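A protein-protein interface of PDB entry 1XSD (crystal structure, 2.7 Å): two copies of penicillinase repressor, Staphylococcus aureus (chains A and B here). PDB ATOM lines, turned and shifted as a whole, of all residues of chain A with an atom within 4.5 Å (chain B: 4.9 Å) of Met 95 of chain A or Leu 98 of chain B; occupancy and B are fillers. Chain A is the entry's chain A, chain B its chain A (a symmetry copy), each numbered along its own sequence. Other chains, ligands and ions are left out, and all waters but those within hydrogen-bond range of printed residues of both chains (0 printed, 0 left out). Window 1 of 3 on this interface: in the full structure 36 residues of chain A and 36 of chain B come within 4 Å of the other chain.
Of the 13 printed residues of chain B, 5 touch a printed residue of chain A.
Printed residues of chain B that touch a printed residue of chain A: Phe 86, Tyr 91, Met 95, Leu 98 and Leu 116.
Hydrophobic or aromatic side chains of chain B within 4 Å of the printed part of chain A: Phe 86, Tyr 91, Met 95, Leu 98 and Leu 116.
Of the 9 printed residues of chain A, 4 touch a printed residue of chain B.
Printed residues of chain A that touch a printed residue of chain B: Ala 83, Met 95, Lys 96 and Leu 98.
Among the printed residues, no Asp or Glu carboxylate lies within 4 Å of a Lys or Arg side-chain nitrogen of the other chain.
Met 95 of chain B touches its own counterpart, Met 95 of chain A.
Met 95 of chain A touches Leu 98 of chain B, and with the chains exchanged Leu 98 of chain A touches Met 95 of chain B.
7 positions are printed for both chains.
Of the 6 pairs that touch across the chains among the printed residues, 3 have their exchanged pair printed and touching as well.
Met 95 of chain A touches two residues of chain B.
Leu 98 of chain B touches just one residue of chain A: Met 95.
Printed residues of chain B within 4 Å of Leu 98 of chain A: Met 95.
Of the printed residues of chain B, Lys 96 of chain A touches Leu 116.
Printed residues of chain A within 4 Å of Phe 86 of chain B: Ala 83 (3.5 Å).
Asp 94 of chain B touches none of the printed residues of chain A.
The nearest residue of chain A that does not touch Leu 98 of chain B is Ala 83 of chain A (4.3 Å).
The side-chain carboxylate of Asp 94 of chain A is in salt-bridge range of the side-chain amino group of Lys 96 of chain A (2.6 Å).
The side-chain hydroxyl of Tyr 91 of chain B is in hydrogen-bond range of the side-chain amide nitrogen of Asn 101 of chain B (3.5 Å).
Among the printed residues, pairs that only touch across the chains: Ala 83 of chain A with Phe 86 of chain B, Ala 83 of chain A with Tyr 91 of chain B, Met 95 of chain A with Met 95 of chain B, Met 95 of chain A with Leu 98 of chain B, Lys 96 of chain A with Leu 116 of chain B and Leu 98 of chain A with Met 95 of chain B.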
ATOM      1  N   ALA A  83      25.501  13.901  35.368  1.00  0.00           N
ATOM      2  CA  ALA A  83      24.667  13.488  34.260  1.00  0.00           C
ATOM      3  C   ALA A  83      23.589  12.447  34.677  1.00  0.00           C
ATOM      4  O   ALA A  83      22.442  12.566  34.241  1.00  0.00           O
ATOM      5  CB  ALA A  83      25.554  12.940  33.113  1.00  0.00           C
ATOM      6  N   LEU A  87      19.764  13.200  34.122  1.00  0.00           N
ATOM      7  CA  LEU A  87      18.925  12.291  33.352  1.00  0.00           C
ATOM      8  C   LEU A  87      17.723  11.707  34.178  1.00  0.00           C
ATOM      9  O   LEU A  87      16.606  11.537  33.683  1.00  0.00           O
ATOM     10  CB  LEU A  87      19.819  11.180  32.814  1.00  0.00           C
ATOM     11  CG  LEU A  87      19.655  10.828  31.336  1.00  0.00           C
ATOM     12  CD1 LEU A  87      18.244  10.386  31.138  1.00  0.00           C
ATOM     13  CD2 LEU A  87      19.984  11.993  30.426  1.00  0.00           C
ATOM     14  N   GLY A  93      16.113   8.849  33.906  1.00  0.00           N
ATOM     15  CA  GLY A  93      17.324   8.212  33.435  1.00  0.00           C
ATOM     16  C   GLY A  93      17.187   7.368  32.189  1.00  0.00           C
ATOM     17  O   GLY A  93      17.346   6.173  32.252  1.00  0.00           O
ATOM     18  N   ASP A  94      16.885   7.975  31.053  1.00  0.00           N
ATOM     19  CA  ASP A  94      16.762   7.229  29.810  1.00  0.00           C
ATOM     20  C   ASP A  94      17.419   8.037  28.698  1.00  0.00           C
ATOM     21  O   ASP A  94      16.832   9.010  28.187  1.00  0.00           O
ATOM     22  CB  ASP A  94      15.290   6.990  29.480  1.00  0.00           C
ATOM     23  CG  ASP A  94      15.100   6.001  28.324  1.00  0.00           C
ATOM     24  OD1 ASP A  94      16.075   5.846  27.521  1.00  0.00           O
ATOM     25  OD2 ASP A  94      13.977   5.403  28.229  1.00  0.00           O
ATOM     26  N   MET A  95      18.648   7.663  28.336  1.00  0.00           N
ATOM     27  CA  MET A  95      19.339   8.385  27.272  1.00  0.00           C
ATOM     28  C   MET A  95      18.447   8.463  26.035  1.00  0.00           C
ATOM     29  O   MET A  95      18.470   9.456  25.299  1.00  0.00           O
ATOM     30  CB  MET A  95      20.651   7.705  26.870  1.00  0.00           C
ATOM     31  CG  MET A  95      21.877   8.310  27.503  1.00  0.00           C
ATOM     32  SD  MET A  95      21.964  10.004  27.236  1.00  0.00           S
ATOM     33  CE  MET A  95      23.089  10.158  26.051  1.00  0.00           C
ATOM     34  N   LYS A  96      17.677   7.408  25.795  1.00  0.00           N
ATOM     35  CA  LYS A  96      16.811   7.418  24.632  1.00  0.00           C
ATOM     36  C   LYS A  96      15.871   8.616  24.736  1.00  0.00           C
ATOM     37  O   LYS A  96      15.843   9.507  23.865  1.00  0.00           O
ATOM     38  CB  LYS A  96      16.026   6.096  24.548  1.00  0.00           C
ATOM     39  CG  LYS A  96      16.931   4.847  24.381  1.00  0.00           C
ATOM     40  CD  LYS A  96      16.144   3.534  24.548  1.00  0.00           C
ATOM     41  CE  LYS A  96      15.620   3.346  25.985  1.00  0.00           C
ATOM     42  NZ  LYS A  96      16.748   3.438  26.964  1.00  0.00           N
ATOM     43  N   SER A  97      15.138   8.636  25.841  1.00  0.00           N
ATOM     44  CA  SER A  97      14.189   9.692  26.080  1.00  0.00           C
ATOM     45  C   SER A  97      14.787  11.084  25.955  1.00  0.00           C
ATOM     46  O   SER A  97      14.078  12.019  25.617  1.00  0.00           O
ATOM     47  CB  SER A  97      13.542   9.516  27.443  1.00  0.00           C
ATOM     48  OG  SER A  97      12.557  10.520  27.630  1.00  0.00           O
ATOM     49  N   LEU A  98      16.084  11.219  26.230  1.00  0.00           N
ATOM     50  CA  LEU A  98      16.769  12.498  26.112  1.00  0.00           C
ATOM     51  C   LEU A  98      17.300  12.706  24.688  1.00  0.00           C
ATOM     52  O   LEU A  98      17.349  13.833  24.167  1.00  0.00           O
ATOM     53  CB  LEU A  98      17.911  12.557  27.117  1.00  0.00           C
ATOM     54  CG  LEU A  98      19.015  13.638  27.122  1.00  0.00           C
ATOM     55  CD1 LEU A  98      20.222  13.179  26.344  1.00  0.00           C
ATOM     56  CD2 LEU A  98      18.493  14.945  26.572  1.00  0.00           C
ATOM     57  N   VAL A  99      17.703  11.631  24.033  1.00  0.00           N
ATOM     58  CA  VAL A  99      18.191  11.821  22.685  1.00  0.00           C
ATOM     59  C   VAL A  99      16.979  12.049  21.784  1.00  0.00           C
ATOM     60  O   VAL A  99      17.045  12.743  20.769  1.00  0.00           O
ATOM     61  CB  VAL A  99      18.996  10.627  22.195  1.00  0.00           C
ATOM     62  CG1 VAL A  99      18.080   9.540  21.762  1.00  0.00           C
ATOM     63  CG2 VAL A  99      19.895  11.065  21.070  1.00  0.00           C
ATOM     64  N   PHE B  86      23.204  22.035  30.736  1.00  0.00           N
ATOM     65  CA  PHE B  86      23.943  20.936  31.302  1.00  0.00           C
ATOM     66  C   PHE B  86      25.050  20.480  30.345  1.00  0.00           C
ATOM     67  O   PHE B  86      26.223  20.407  30.725  1.00  0.00           O
ATOM     68  CB  PHE B  86      22.967  19.818  31.561  1.00  0.00           C
ATOM     69  CG  PHE B  86      23.582  18.494  31.574  1.00  0.00           C
ATOM     70  CD1 PHE B  86      24.242  18.041  32.706  1.00  0.00           C
ATOM     71  CD2 PHE B  86      23.507  17.684  30.454  1.00  0.00           C
ATOM     72  CE1 PHE B  86      24.836  16.765  32.736  1.00  0.00           C
ATOM     73  CE2 PHE B  86      24.083  16.418  30.449  1.00  0.00           C
ATOM     74  CZ  PHE B  86      24.755  15.947  31.599  1.00  0.00           C
ATOM     75  N   LEU B  87      24.677  20.177  29.104  1.00  0.00           N
ATOM     76  CA  LEU B  87      25.633  19.728  28.100  1.00  0.00           C
ATOM     77  C   LEU B  87      26.797  20.753  27.850  1.00  0.00           C
ATOM     78  O   LEU B  87      27.960  20.392  27.651  1.00  0.00           O
ATOM     79  CB  LEU B  87      24.859  19.445  26.818  1.00  0.00           C
ATOM     80  CG  LEU B  87      25.167  18.125  26.112  1.00  0.00           C
ATOM     81  CD1 LEU B  87      26.615  18.141  25.753  1.00  0.00           C
ATOM     82  CD2 LEU B  87      24.842  16.922  26.972  1.00  0.00           C
ATOM     83  N   TYR B  91      30.031  19.209  28.837  1.00  0.00           N
ATOM     84  CA  TYR B  91      30.640  18.651  27.624  1.00  0.00           C
ATOM     85  C   TYR B  91      30.786  19.621  26.463  1.00  0.00           C
ATOM     86  O   TYR B  91      30.922  19.176  25.325  1.00  0.00           O
ATOM     87  CB  TYR B  91      29.826  17.450  27.152  1.00  0.00           C
ATOM     88  CG  TYR B  91      29.546  16.408  28.225  1.00  0.00           C
ATOM     89  CD1 TYR B  91      30.445  15.365  28.481  1.00  0.00           C
ATOM     90  CD2 TYR B  91      28.393  16.466  28.986  1.00  0.00           C
ATOM     91  CE1 TYR B  91      30.197  14.404  29.478  1.00  0.00           C
ATOM     92  CE2 TYR B  91      28.128  15.524  29.984  1.00  0.00           C
ATOM     93  CZ  TYR B  91      29.033  14.499  30.235  1.00  0.00           C
ATOM     94  OH  TYR B  91      28.805  13.632  31.291  1.00  0.00           O
ATOM     95  N   ASP B  94      28.127  18.779  23.523  1.00  0.00           N
ATOM     96  CA  ASP B  94      28.399  17.786  22.495  1.00  0.00           C
ATOM     97  C   ASP B  94      27.787  16.461  22.932  1.00  0.00           C
ATOM     98  O   ASP B  94      28.351  15.751  23.786  1.00  0.00           O
ATOM     99  CB  ASP B  94      29.907  17.624  22.302  1.00  0.00           C
ATOM    100  CG  ASP B  94      30.254  16.783  21.068  1.00  0.00           C
ATOM    101  OD1 ASP B  94      29.361  15.989  20.631  1.00  0.00           O
ATOM    102  OD2 ASP B  94      31.416  16.920  20.561  1.00  0.00           O
ATOM    103  N   MET B  95      26.619  16.133  22.377  1.00  0.00           N
ATOM    104  CA  MET B  95      25.974  14.874  22.740  1.00  0.00           C
ATOM    105  C   MET B  95      26.958  13.719  22.571  1.00  0.00           C
ATOM    106  O   MET B  95      26.934  12.749  23.336  1.00  0.00           O
ATOM    107  CB  MET B  95      24.746  14.582  21.874  1.00  0.00           C
ATOM    108  CG  MET B  95      23.435  14.956  22.517  1.00  0.00           C
ATOM    109  SD  MET B  95      23.264  14.247  24.072  1.00  0.00           S
ATOM    110  CE  MET B  95      22.233  12.995  23.822  1.00  0.00           C
ATOM    111  N   LYS B  96      27.811  13.815  21.558  1.00  0.00           N
ATOM    112  CA  LYS B  96      28.768  12.747  21.340  1.00  0.00           C
ATOM    113  C   LYS B  96      29.619  12.593  22.598  1.00  0.00           C
ATOM    114  O   LYS B  96      29.662  11.521  23.234  1.00  0.00           O
ATOM    115  CB  LYS B  96      29.640  13.064  20.110  1.00  0.00           C
ATOM    116  CG  LYS B  96      28.833  13.174  18.790  1.00  0.00           C
ATOM    117  CD  LYS B  96      29.685  13.730  17.634  1.00  0.00           C
ATOM    118  CE  LYS B  96      30.099  15.196  17.867  1.00  0.00           C
ATOM    119  NZ  LYS B  96      28.890  16.043  18.113  1.00  0.00           N
ATOM    120  N   SER B  97      30.254  13.697  22.963  1.00  0.00           N
ATOM    121  CA  SER B  97      31.111  13.711  24.119  1.00  0.00           C
ATOM    122  C   SER B  97      30.439  13.187  25.378  1.00  0.00           C
ATOM    123  O   SER B  97      31.113  12.661  26.250  1.00  0.00           O
ATOM    124  CB  SER B  97      31.654  15.111  24.354  1.00  0.00           C
ATOM    125  OG  SER B  97      32.553  15.089  25.451  1.00  0.00           O
ATOM    126  N   LEU B  98      29.118  13.334  25.471  1.00  0.00           N
ATOM    127  CA  LEU B  98      28.365  12.840  26.615  1.00  0.00           C
ATOM    128  C   LEU B  98      27.942  11.380  26.404  1.00  0.00           C
ATOM    129  O   LEU B  98      27.865  10.580  27.352  1.00  0.00           O
ATOM    130  CB  LEU B  98      27.141  13.719  26.836  1.00  0.00           C
ATOM    131  CG  LEU B  98      25.975  13.370  27.786  1.00  0.00           C
ATOM    132  CD1 LEU B  98      24.868  12.665  27.044  1.00  0.00           C
ATOM    133  CD2 LEU B  98      26.457  12.530  28.946  1.00  0.00           C
ATOM    134  N   VAL B  99      27.664  11.007  25.168  1.00  0.00           N
ATOM    135  CA  VAL B  99      27.278   9.628  24.963  1.00  0.00           C
ATOM    136  C   VAL B  99      28.543   8.778  25.052  1.00  0.00           C
ATOM    137  O   VAL B  99      28.518   7.614  25.453  1.00  0.00           O
ATOM    138  CB  VAL B  99      26.593   9.420  23.621  1.00  0.00           C
ATOM    139  CG1 VAL B  99      27.610   9.346  22.539  1.00  0.00           C
ATOM    140  CG2 VAL B  99      25.765   8.164  23.679  1.00  0.00           C
ATOM    141  N   LEU B 100      29.671   9.374  24.709  1.00  0.00           N
ATOM    142  CA  LEU B 100      30.910   8.641  24.805  1.00  0.00           C
ATOM    143  C   LEU B 100      31.366   8.490  26.277  1.00  0.00           C
ATOM    144  O   LEU B 100      31.938   7.467  26.641  1.00  0.00           O
ATOM    145  CB  LEU B 100      31.971   9.338  23.956  1.00  0.00           C
ATOM    146  CG  LEU B 100      33.128   8.400  23.650  1.00  0.00           C
ATOM    147  CD1 LEU B 100      32.545   6.997  23.355  1.00  0.00           C
ATOM    148  CD2 LEU B 100      34.000   8.968  22.498  1.00  0.00           C
ATOM    149  N   ASN B 101      31.121   9.505  27.112  1.00  0.00           N
ATOM    150  CA  ASN B 101      31.483   9.450  28.529  1.00  0.00           C
ATOM    151  C   ASN B 101      30.605   8.344  29.146  1.00  0.00           C
ATOM    152  O   ASN B 101      30.990   7.690  30.108  1.00  0.00           O
ATOM    153  CB  ASN B 101      31.228  10.826  29.187  1.00  0.00           C
ATOM    154  CG  ASN B 101      31.138  10.771  30.765  1.00  0.00           C
ATOM    155  OD1 ASN B 101      30.515   9.856  31.356  1.00  0.00           O
ATOM    156  ND2 ASN B 101      31.727  11.777  31.433  1.00  0.00           N
ATOM    157  N   PHE B 102      29.426   8.121  28.576  1.00  0.00           N
ATOM    158  CA  PHE B 102      28.542   7.088  29.099  1.00  0.00           C
ATOM    159  C   PHE B 102      29.078   5.714  28.848  1.00  0.00           C
ATOM    160  O   PHE B 102      29.290   4.933  29.775  1.00  0.00           O
ATOM    161  CB  PHE B 102      27.167   7.178  28.474  1.00  0.00           C
ATOM    162  CG  PHE B 102      26.130   7.615  29.431  1.00  0.00           C
ATOM    163  CD1 PHE B 102      25.495   6.698  30.224  1.00  0.00           C
ATOM    164  CD2 PHE B 102      25.912   8.968  29.648  1.00  0.00           C
ATOM    165  CE1 PHE B 102      24.667   7.120  31.238  1.00  0.00           C
ATOM    166  CE2 PHE B 102      25.085   9.413  30.663  1.00  0.00           C
ATOM    167  CZ  PHE B 102      24.463   8.498  31.466  1.00  0.00           C
ATOM    168  N   LEU B 116      19.719   2.022  21.848  1.00  0.00           N
ATOM    169  CA  LEU B 116      20.011   3.396  21.504  1.00  0.00           C
ATOM    170  C   LEU B 116      20.351   3.444  20.022  1.00  0.00           C
ATOM    171  O   LEU B 116      19.569   3.966  19.225  1.00  0.00           O
ATOM    172  CB  LEU B 116      21.174   3.924  22.335  1.00  0.00           C
ATOM    173  CG  LEU B 116      21.087   5.435  22.509  1.00  0.00           C
ATOM    174  CD1 LEU B 116      19.802   5.819  23.243  1.00  0.00           C
ATOM    175  CD2 LEU B 116      22.286   5.898  23.270  1.00  0.00           C
